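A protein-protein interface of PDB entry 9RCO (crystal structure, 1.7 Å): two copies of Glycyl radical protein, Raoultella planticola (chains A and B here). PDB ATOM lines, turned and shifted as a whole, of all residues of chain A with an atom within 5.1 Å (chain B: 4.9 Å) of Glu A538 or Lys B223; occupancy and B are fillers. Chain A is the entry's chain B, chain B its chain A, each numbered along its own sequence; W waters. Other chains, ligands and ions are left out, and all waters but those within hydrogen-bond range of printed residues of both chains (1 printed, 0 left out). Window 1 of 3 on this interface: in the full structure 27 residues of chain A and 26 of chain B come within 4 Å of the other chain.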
ATOM      1  N   ALA A  70     -10.571  -8.582 -22.683  1.00  0.00           N
ATOM      2  CA  ALA A  70     -11.965  -8.318 -23.045  1.00  0.00           C
ATOM      3  C   ALA A  70     -12.306  -6.826 -23.080  1.00  0.00           C
ATOM      4  O   ALA A  70     -13.045  -6.376 -23.965  1.00  0.00           O
ATOM      5  CB  ALA A  70     -12.891  -9.049 -22.073  1.00  0.00           C
ATOM      6  N   LEU A 157     -21.492 -18.914 -21.674  1.00  0.00           N
ATOM      7  CA  LEU A 157     -20.638 -18.996 -20.494  1.00  0.00           C
ATOM      8  C   LEU A 157     -21.460 -19.018 -19.208  1.00  0.00           C
ATOM      9  O   LEU A 157     -21.190 -19.820 -18.305  1.00  0.00           O
ATOM     10  CB  LEU A 157     -19.661 -17.822 -20.475  1.00  0.00           C
ATOM     11  CG  LEU A 157     -18.694 -17.731 -19.289  1.00  0.00           C
ATOM     12  CD1 LEU A 157     -17.778 -18.959 -19.220  1.00  0.00           C
ATOM     13  CD2 LEU A 157     -17.864 -16.464 -19.368  1.00  0.00           C
ATOM     14  N   TYR A 161     -21.658 -21.919 -15.825  1.00  0.00           N
ATOM     15  CA  TYR A 161     -21.379 -21.755 -14.406  1.00  0.00           C
ATOM     16  C   TYR A 161     -22.506 -22.263 -13.512  1.00  0.00           C
ATOM     17  O   TYR A 161     -22.261 -22.516 -12.325  1.00  0.00           O
ATOM     18  CB  TYR A 161     -21.125 -20.285 -14.076  1.00  0.00           C
ATOM     19  CG  TYR A 161     -19.734 -19.762 -14.379  1.00  0.00           C
ATOM     20  CD1 TYR A 161     -18.629 -20.249 -13.693  1.00  0.00           C
ATOM     21  CD2 TYR A 161     -19.543 -18.733 -15.295  1.00  0.00           C
ATOM     22  CE1 TYR A 161     -17.359 -19.759 -13.936  1.00  0.00           C
ATOM     23  CE2 TYR A 161     -18.268 -18.226 -15.547  1.00  0.00           C
ATOM     24  CZ  TYR A 161     -17.178 -18.753 -14.865  1.00  0.00           C
ATOM     25  OH  TYR A 161     -15.908 -18.267 -15.098  1.00  0.00           O
ATOM     26  N   ILE A 534     -21.025 -13.050 -13.407  1.00  0.00           N
ATOM     27  CA  ILE A 534     -19.641 -13.413 -13.691  1.00  0.00           C
ATOM     28  C   ILE A 534     -19.391 -13.409 -15.193  1.00  0.00           C
ATOM     29  O   ILE A 534     -18.411 -12.833 -15.672  1.00  0.00           O
ATOM     30  CB  ILE A 534     -19.306 -14.780 -13.070  1.00  0.00           C
ATOM     31  CG1 ILE A 534     -19.321 -14.691 -11.538  1.00  0.00           C
ATOM     32  CG2 ILE A 534     -17.934 -15.281 -13.570  1.00  0.00           C
ATOM     33  CD1 ILE A 534     -19.365 -16.059 -10.847  1.00  0.00           C
ATOM     34  N   ALA A 535     -20.274 -14.047 -15.961  1.00  0.00           N
ATOM     35  CA  ALA A 535     -20.083 -14.125 -17.412  1.00  0.00           C
ATOM     36  C   ALA A 535     -19.963 -12.740 -18.053  1.00  0.00           C
ATOM     37  O   ALA A 535     -19.105 -12.521 -18.923  1.00  0.00           O
ATOM     38  CB  ALA A 535     -21.226 -14.915 -18.048  1.00  0.00           C
ATOM     39  N   HIS A 536     -20.797 -11.782 -17.638  1.00  0.00           N
ATOM     40  CA  HIS A 536     -20.668 -10.437 -18.203  1.00  0.00           C
ATOM     41  C   HIS A 536     -19.333  -9.802 -17.821  1.00  0.00           C
ATOM     42  O   HIS A 536     -18.695  -9.124 -18.643  1.00  0.00           O
ATOM     43  CB  HIS A 536     -21.834  -9.553 -17.752  1.00  0.00           C
ATOM     44  CG  HIS A 536     -23.070  -9.728 -18.575  1.00  0.00           C
ATOM     45  ND1 HIS A 536     -23.274  -9.038 -19.750  1.00  0.00           N
ATOM     46  CD2 HIS A 536     -24.156 -10.521 -18.408  1.00  0.00           C
ATOM     47  CE1 HIS A 536     -24.441  -9.385 -20.265  1.00  0.00           C
ATOM     48  NE2 HIS A 536     -24.998 -10.280 -19.467  1.00  0.00           N
ATOM     49  N   GLY A 537     -18.894 -10.010 -16.578  1.00  0.00           N
ATOM     50  CA  GLY A 537     -17.618  -9.463 -16.160  1.00  0.00           C
ATOM     51  C   GLY A 537     -16.444 -10.042 -16.925  1.00  0.00           C
ATOM     52  O   GLY A 537     -15.479  -9.332 -17.220  1.00  0.00           O
ATOM     53  N   GLU A 538     -16.509 -11.336 -17.265  1.00  0.00           N
ATOM     54  CA  GLU A 538     -15.377 -11.985 -17.931  1.00  0.00           C
ATOM     55  C   GLU A 538     -15.376 -11.737 -19.427  1.00  0.00           C
ATOM     56  O   GLU A 538     -14.302 -11.648 -20.026  1.00  0.00           O
ATOM     57  CB  GLU A 538     -15.363 -13.502 -17.680  1.00  0.00           C
ATOM     58  CG  GLU A 538     -15.750 -13.922 -16.272  1.00  0.00           C
ATOM     59  CD  GLU A 538     -15.196 -15.280 -15.877  1.00  0.00           C
ATOM     60  OE1 GLU A 538     -15.480 -16.261 -16.594  1.00  0.00           O
ATOM     61  OE2 GLU A 538     -14.532 -15.367 -14.815  1.00  0.00           O
ATOM     62  N   ARG A 539     -16.547 -11.628 -20.051  1.00  0.00           N
ATOM     63  CA  ARG A 539     -16.610 -11.531 -21.501  1.00  0.00           C
ATOM     64  C   ARG A 539     -17.102 -10.197 -22.020  1.00  0.00           C
ATOM     65  O   ARG A 539     -16.819  -9.878 -23.175  1.00  0.00           O
ATOM     66  CB  ARG A 539     -17.501 -12.643 -22.069  1.00  0.00           C
ATOM     67  CG  ARG A 539     -16.826 -13.991 -22.036  1.00  0.00           C
ATOM     68  CD  ARG A 539     -17.633 -15.102 -22.726  1.00  0.00           C
ATOM     69  NE  ARG A 539     -16.812 -16.309 -22.813  1.00  0.00           N
ATOM     70  CZ  ARG A 539     -17.144 -17.412 -23.474  1.00  0.00           C
ATOM     71  NH1 ARG A 539     -18.309 -17.494 -24.120  1.00  0.00           N
ATOM     72  NH2 ARG A 539     -16.300 -18.427 -23.496  1.00  0.00           N
ATOM     73  N   CYS A 540     -17.845  -9.415 -21.233  1.00  0.00           N
ATOM     74  CA  CYS A 540     -18.368  -8.215 -21.877  1.00  0.00           C
ATOM     75  C   CYS A 540     -18.380  -7.010 -20.932  1.00  0.00           C
ATOM     76  O   CYS A 540     -19.426  -6.352 -20.758  1.00  0.00           O
ATOM     77  CB  CYS A 540     -19.758  -8.505 -22.448  1.00  0.00           C
ATOM     78  SG  CYS A 540     -20.284  -7.263 -23.694  1.00  0.00           S
ATOM     79  N   PRO A 541     -17.230  -6.642 -20.355  1.00  0.00           N
ATOM     80  CA  PRO A 541     -17.153  -5.362 -19.639  1.00  0.00           C
ATOM     81  C   PRO A 541     -17.199  -4.204 -20.633  1.00  0.00           C
ATOM     82  O   PRO A 541     -16.632  -4.281 -21.727  1.00  0.00           O
ATOM     83  CB  PRO A 541     -15.795  -5.445 -18.919  1.00  0.00           C
ATOM     84  CG  PRO A 541     -14.947  -6.237 -19.865  1.00  0.00           C
ATOM     85  CD  PRO A 541     -15.896  -7.288 -20.445  1.00  0.00           C
ATOM     86  N   SER B 219     -21.036 -15.366  -3.432  1.00  0.00           N
ATOM     87  CA  SER B 219     -20.862 -15.714  -4.840  1.00  0.00           C
ATOM     88  C   SER B 219     -19.535 -16.417  -5.123  1.00  0.00           C
ATOM     89  O   SER B 219     -19.370 -16.973  -6.218  1.00  0.00           O
ATOM     90  CB  SER B 219     -20.982 -14.467  -5.713  1.00  0.00           C
ATOM     91  OG  SER B 219     -19.990 -13.510  -5.383  1.00  0.00           O
ATOM     92  N   ASP B 220     -18.616 -16.449  -4.157  1.00  0.00           N
ATOM     93  CA  ASP B 220     -17.273 -16.991  -4.350  1.00  0.00           C
ATOM     94  C   ASP B 220     -17.264 -18.481  -4.657  1.00  0.00           C
ATOM     95  O   ASP B 220     -16.284 -18.989  -5.212  1.00  0.00           O
ATOM     96  CB  ASP B 220     -16.426 -16.768  -3.093  1.00  0.00           C
ATOM     97  CG  ASP B 220     -15.892 -15.355  -2.975  1.00  0.00           C
ATOM     98  OD1 ASP B 220     -15.995 -14.578  -3.946  1.00  0.00           O
ATOM     99  OD2 ASP B 220     -15.349 -15.036  -1.892  1.00  0.00           O
ATOM    100  N   TYR B 221     -18.303 -19.214  -4.246  1.00  0.00           N
ATOM    101  CA  TYR B 221     -18.271 -20.660  -4.427  1.00  0.00           C
ATOM    102  C   TYR B 221     -18.399 -21.064  -5.881  1.00  0.00           C
ATOM    103  O   TYR B 221     -17.966 -22.160  -6.242  1.00  0.00           O
ATOM    104  CB  TYR B 221     -19.368 -21.297  -3.574  1.00  0.00           C
ATOM    105  CG  TYR B 221     -20.763 -21.342  -4.176  1.00  0.00           C
ATOM    106  CD1 TYR B 221     -21.189 -22.361  -5.034  1.00  0.00           C
ATOM    107  CD2 TYR B 221     -21.668 -20.322  -3.871  1.00  0.00           C
ATOM    108  CE1 TYR B 221     -22.492 -22.355  -5.556  1.00  0.00           C
ATOM    109  CE2 TYR B 221     -22.946 -20.313  -4.376  1.00  0.00           C
ATOM    110  CZ  TYR B 221     -23.360 -21.316  -5.216  1.00  0.00           C
ATOM    111  OH  TYR B 221     -24.654 -21.241  -5.686  1.00  0.00           O
ATOM    112  N   ILE B 222     -18.954 -20.191  -6.720  1.00  0.00           N
ATOM    113  CA  ILE B 222     -19.290 -20.588  -8.081  1.00  0.00           C
ATOM    114  C   ILE B 222     -18.034 -20.947  -8.862  1.00  0.00           C
ATOM    115  O   ILE B 222     -17.970 -21.989  -9.534  1.00  0.00           O
ATOM    116  CB  ILE B 222     -20.084 -19.478  -8.775  1.00  0.00           C
ATOM    117  CG1 ILE B 222     -21.444 -19.312  -8.088  1.00  0.00           C
ATOM    118  CG2 ILE B 222     -20.214 -19.775 -10.278  1.00  0.00           C
ATOM    119  CD1 ILE B 222     -22.174 -18.033  -8.494  1.00  0.00           C
ATOM    120  N   LYS B 223     -17.008 -20.097  -8.782  1.00  0.00           N
ATOM    121  CA  LYS B 223     -15.787 -20.393  -9.512  1.00  0.00           C
ATOM    122  C   LYS B 223     -14.978 -21.498  -8.834  1.00  0.00           C
ATOM    123  O   LYS B 223     -14.342 -22.295  -9.533  1.00  0.00           O
ATOM    124  CB  LYS B 223     -14.944 -19.126  -9.705  1.00  0.00           C
ATOM    125  CG  LYS B 223     -15.508 -18.188 -10.807  1.00  0.00           C
ATOM    126  CD  LYS B 223     -14.675 -16.920 -10.988  1.00  0.00           C
ATOM    127  CE  LYS B 223     -13.362 -17.190 -11.741  1.00  0.00           C
ATOM    128  NZ  LYS B 223     -13.576 -17.491 -13.199  1.00  0.00           N
ATOM    129  N   LYS B 224     -15.023 -21.590  -7.496  1.00  0.00           N
ATOM    130  CA  LYS B 224     -14.327 -22.680  -6.820  1.00  0.00           C
ATOM    131  C   LYS B 224     -14.927 -24.018  -7.208  1.00  0.00           C
ATOM    132  O   LYS B 224     -14.209 -25.015  -7.370  1.00  0.00           O
ATOM    133  CB  LYS B 224     -14.388 -22.500  -5.306  1.00  0.00           C
ATOM    134  CG  LYS B 224     -13.758 -21.206  -4.813  1.00  0.00           C
ATOM    135  CD  LYS B 224     -13.827 -21.153  -3.284  1.00  0.00           C
ATOM    136  CE  LYS B 224     -13.193 -19.887  -2.739  1.00  0.00           C
ATOM    137  NZ  LYS B 224     -13.223 -19.820  -1.239  1.00  0.00           N
ATOM    138  N   GLU B 225     -16.248 -24.061  -7.348  1.00  0.00           N
ATOM    139  CA  GLU B 225     -16.911 -25.290  -7.750  1.00  0.00           C
ATOM    140  C   GLU B 225     -16.503 -25.701  -9.167  1.00  0.00           C
ATOM    141  O   GLU B 225     -16.280 -26.891  -9.433  1.00  0.00           O
ATOM    142  CB  GLU B 225     -18.421 -25.094  -7.614  1.00  0.00           C
ATOM    143  CG  GLU B 225     -19.268 -26.250  -8.040  1.00  0.00           C
ATOM    144  CD  GLU B 225     -20.538 -26.326  -7.214  1.00  0.00           C
ATOM    145  OE1 GLU B 225     -21.327 -25.366  -7.281  1.00  0.00           O
ATOM    146  OE2 GLU B 225     -20.772 -27.358  -6.553  1.00  0.00           O
ATOM    147  N   GLN B 226     -16.386 -24.734 -10.090  1.00  0.00           N
ATOM    148  CA  GLN B 226     -15.854 -25.039 -11.421  1.00  0.00           C
ATOM    149  C   GLN B 226     -14.458 -25.648 -11.332  1.00  0.00           C
ATOM    150  O   GLN B 226     -14.146 -26.619 -12.032  1.00  0.00           O
ATOM    151  CB  GLN B 226     -15.824 -23.785 -12.295  1.00  0.00           C
ATOM    152  CG  GLN B 226     -17.191 -23.290 -12.728  1.00  0.00           C
ATOM    153  CD  GLN B 226     -17.875 -24.231 -13.717  1.00  0.00           C
ATOM    154  OE1 GLN B 226     -17.272 -24.669 -14.708  1.00  0.00           O
ATOM    155  NE2 GLN B 226     -19.119 -24.569 -13.432  1.00  0.00           N
ATOM    156  N   PHE B 227     -13.594 -25.063 -10.498  1.00  0.00           N
ATOM    157  CA  PHE B 227     -12.252 -25.619 -10.309  1.00  0.00           C
ATOM    158  C   PHE B 227     -12.328 -27.054  -9.810  1.00  0.00           C
ATOM    159  O   PHE B 227     -11.675 -27.951 -10.359  1.00  0.00           O
ATOM    160  CB  PHE B 227     -11.462 -24.749  -9.330  1.00  0.00           C
ATOM    161  CG  PHE B 227     -10.131 -25.333  -8.935  1.00  0.00           C
ATOM    162  CD1 PHE B 227      -9.055 -25.301  -9.811  1.00  0.00           C
ATOM    163  CD2 PHE B 227      -9.961 -25.928  -7.690  1.00  0.00           C
ATOM    164  CE1 PHE B 227      -7.832 -25.841  -9.446  1.00  0.00           C
ATOM    165  CE2 PHE B 227      -8.759 -26.475  -7.320  1.00  0.00           C
ATOM    166  CZ  PHE B 227      -7.678 -26.433  -8.193  1.00  0.00           C
ATOM    167  N   GLY B 556      -9.500 -24.004  -3.373  1.00  0.00           N
ATOM    168  CA  GLY B 556     -10.336 -24.001  -4.556  1.00  0.00           C
ATOM    169  C   GLY B 556      -9.819 -23.130  -5.681  1.00  0.00           C
ATOM    170  O   GLY B 556     -10.613 -22.584  -6.450  1.00  0.00           O
HETATM  171  O   HOH W   1     -19.911 -23.396 -10.999  1.00  0.00           O
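Printed residues of chain B within 4 Å of Tyr A161: Ile B222, Lys B223 and Gln B226. Printed residues of chain B within 4 Å of Ile A534: Ile B222 (3.9 Å). Gly A537 touches none of the printed residues of chain B. Glu A538 touches just one residue of chain B: Lys B223 (2.8 Å). Tyr B221 touches none of the printed residues of chain A. Of the printed residues of chain A, Ile B222 touches Tyr A161 (3.8 Å) and Ile A534 (3.9 Å). Of chain A, only Tyr A161 and Glu A538 come within 4 Å of Lys B223. Of the printed residues of chain A, Gln B226 touches Tyr A161. The nearest printed residue of chain B that does not touch Glu A538 is Gln B226 (8.2 Å). The nearest printed residue of chain B that does not touch Tyr A161 is Glu B225 (5.9 Å).
Printed residues of chain B that touch a printed residue of chain A: Ile B222, Lys B223 and Gln B226. Of the 11 printed residues of chain A, 3 touch a printed residue of chain B. Hydrophobic or aromatic side chains of chain A within 4 Å of the printed part of chain B: Tyr A161 and Ile A534.
NZ of Lys B223 sits at hydrogen-bond distance from OH of Tyr A161, at 3.1 Å. The side-chain amino group (NZ) of Lys B223 is in salt-bridge range of the side-chain carboxylate (OE2) of Glu A538, 2.8 Å away.
Tyr A161 touches Ile B222 (CD1 to CG2, 3.8 Å). Tyr A161 touches Gln B226 (CD1 to CG, 3.5 Å). Ile B222 touches Ile A534 (CG2 to CD1, 3.9 Å).
No position is printed for both chains. Of the 5 pairs that touch across the chains among the printed residues, none has its exchanged pair printed and touching as well.
Water W1 lies within hydrogen-bond range of O of Ile B222 (2.8 Å), NE2 of Gln B226 (2.8 Å) and O of Tyr A161 (2.8 Å).
OE1 of Glu A538 lies within hydrogen-bond range of OH of Tyr A161, 2.5 Å away.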
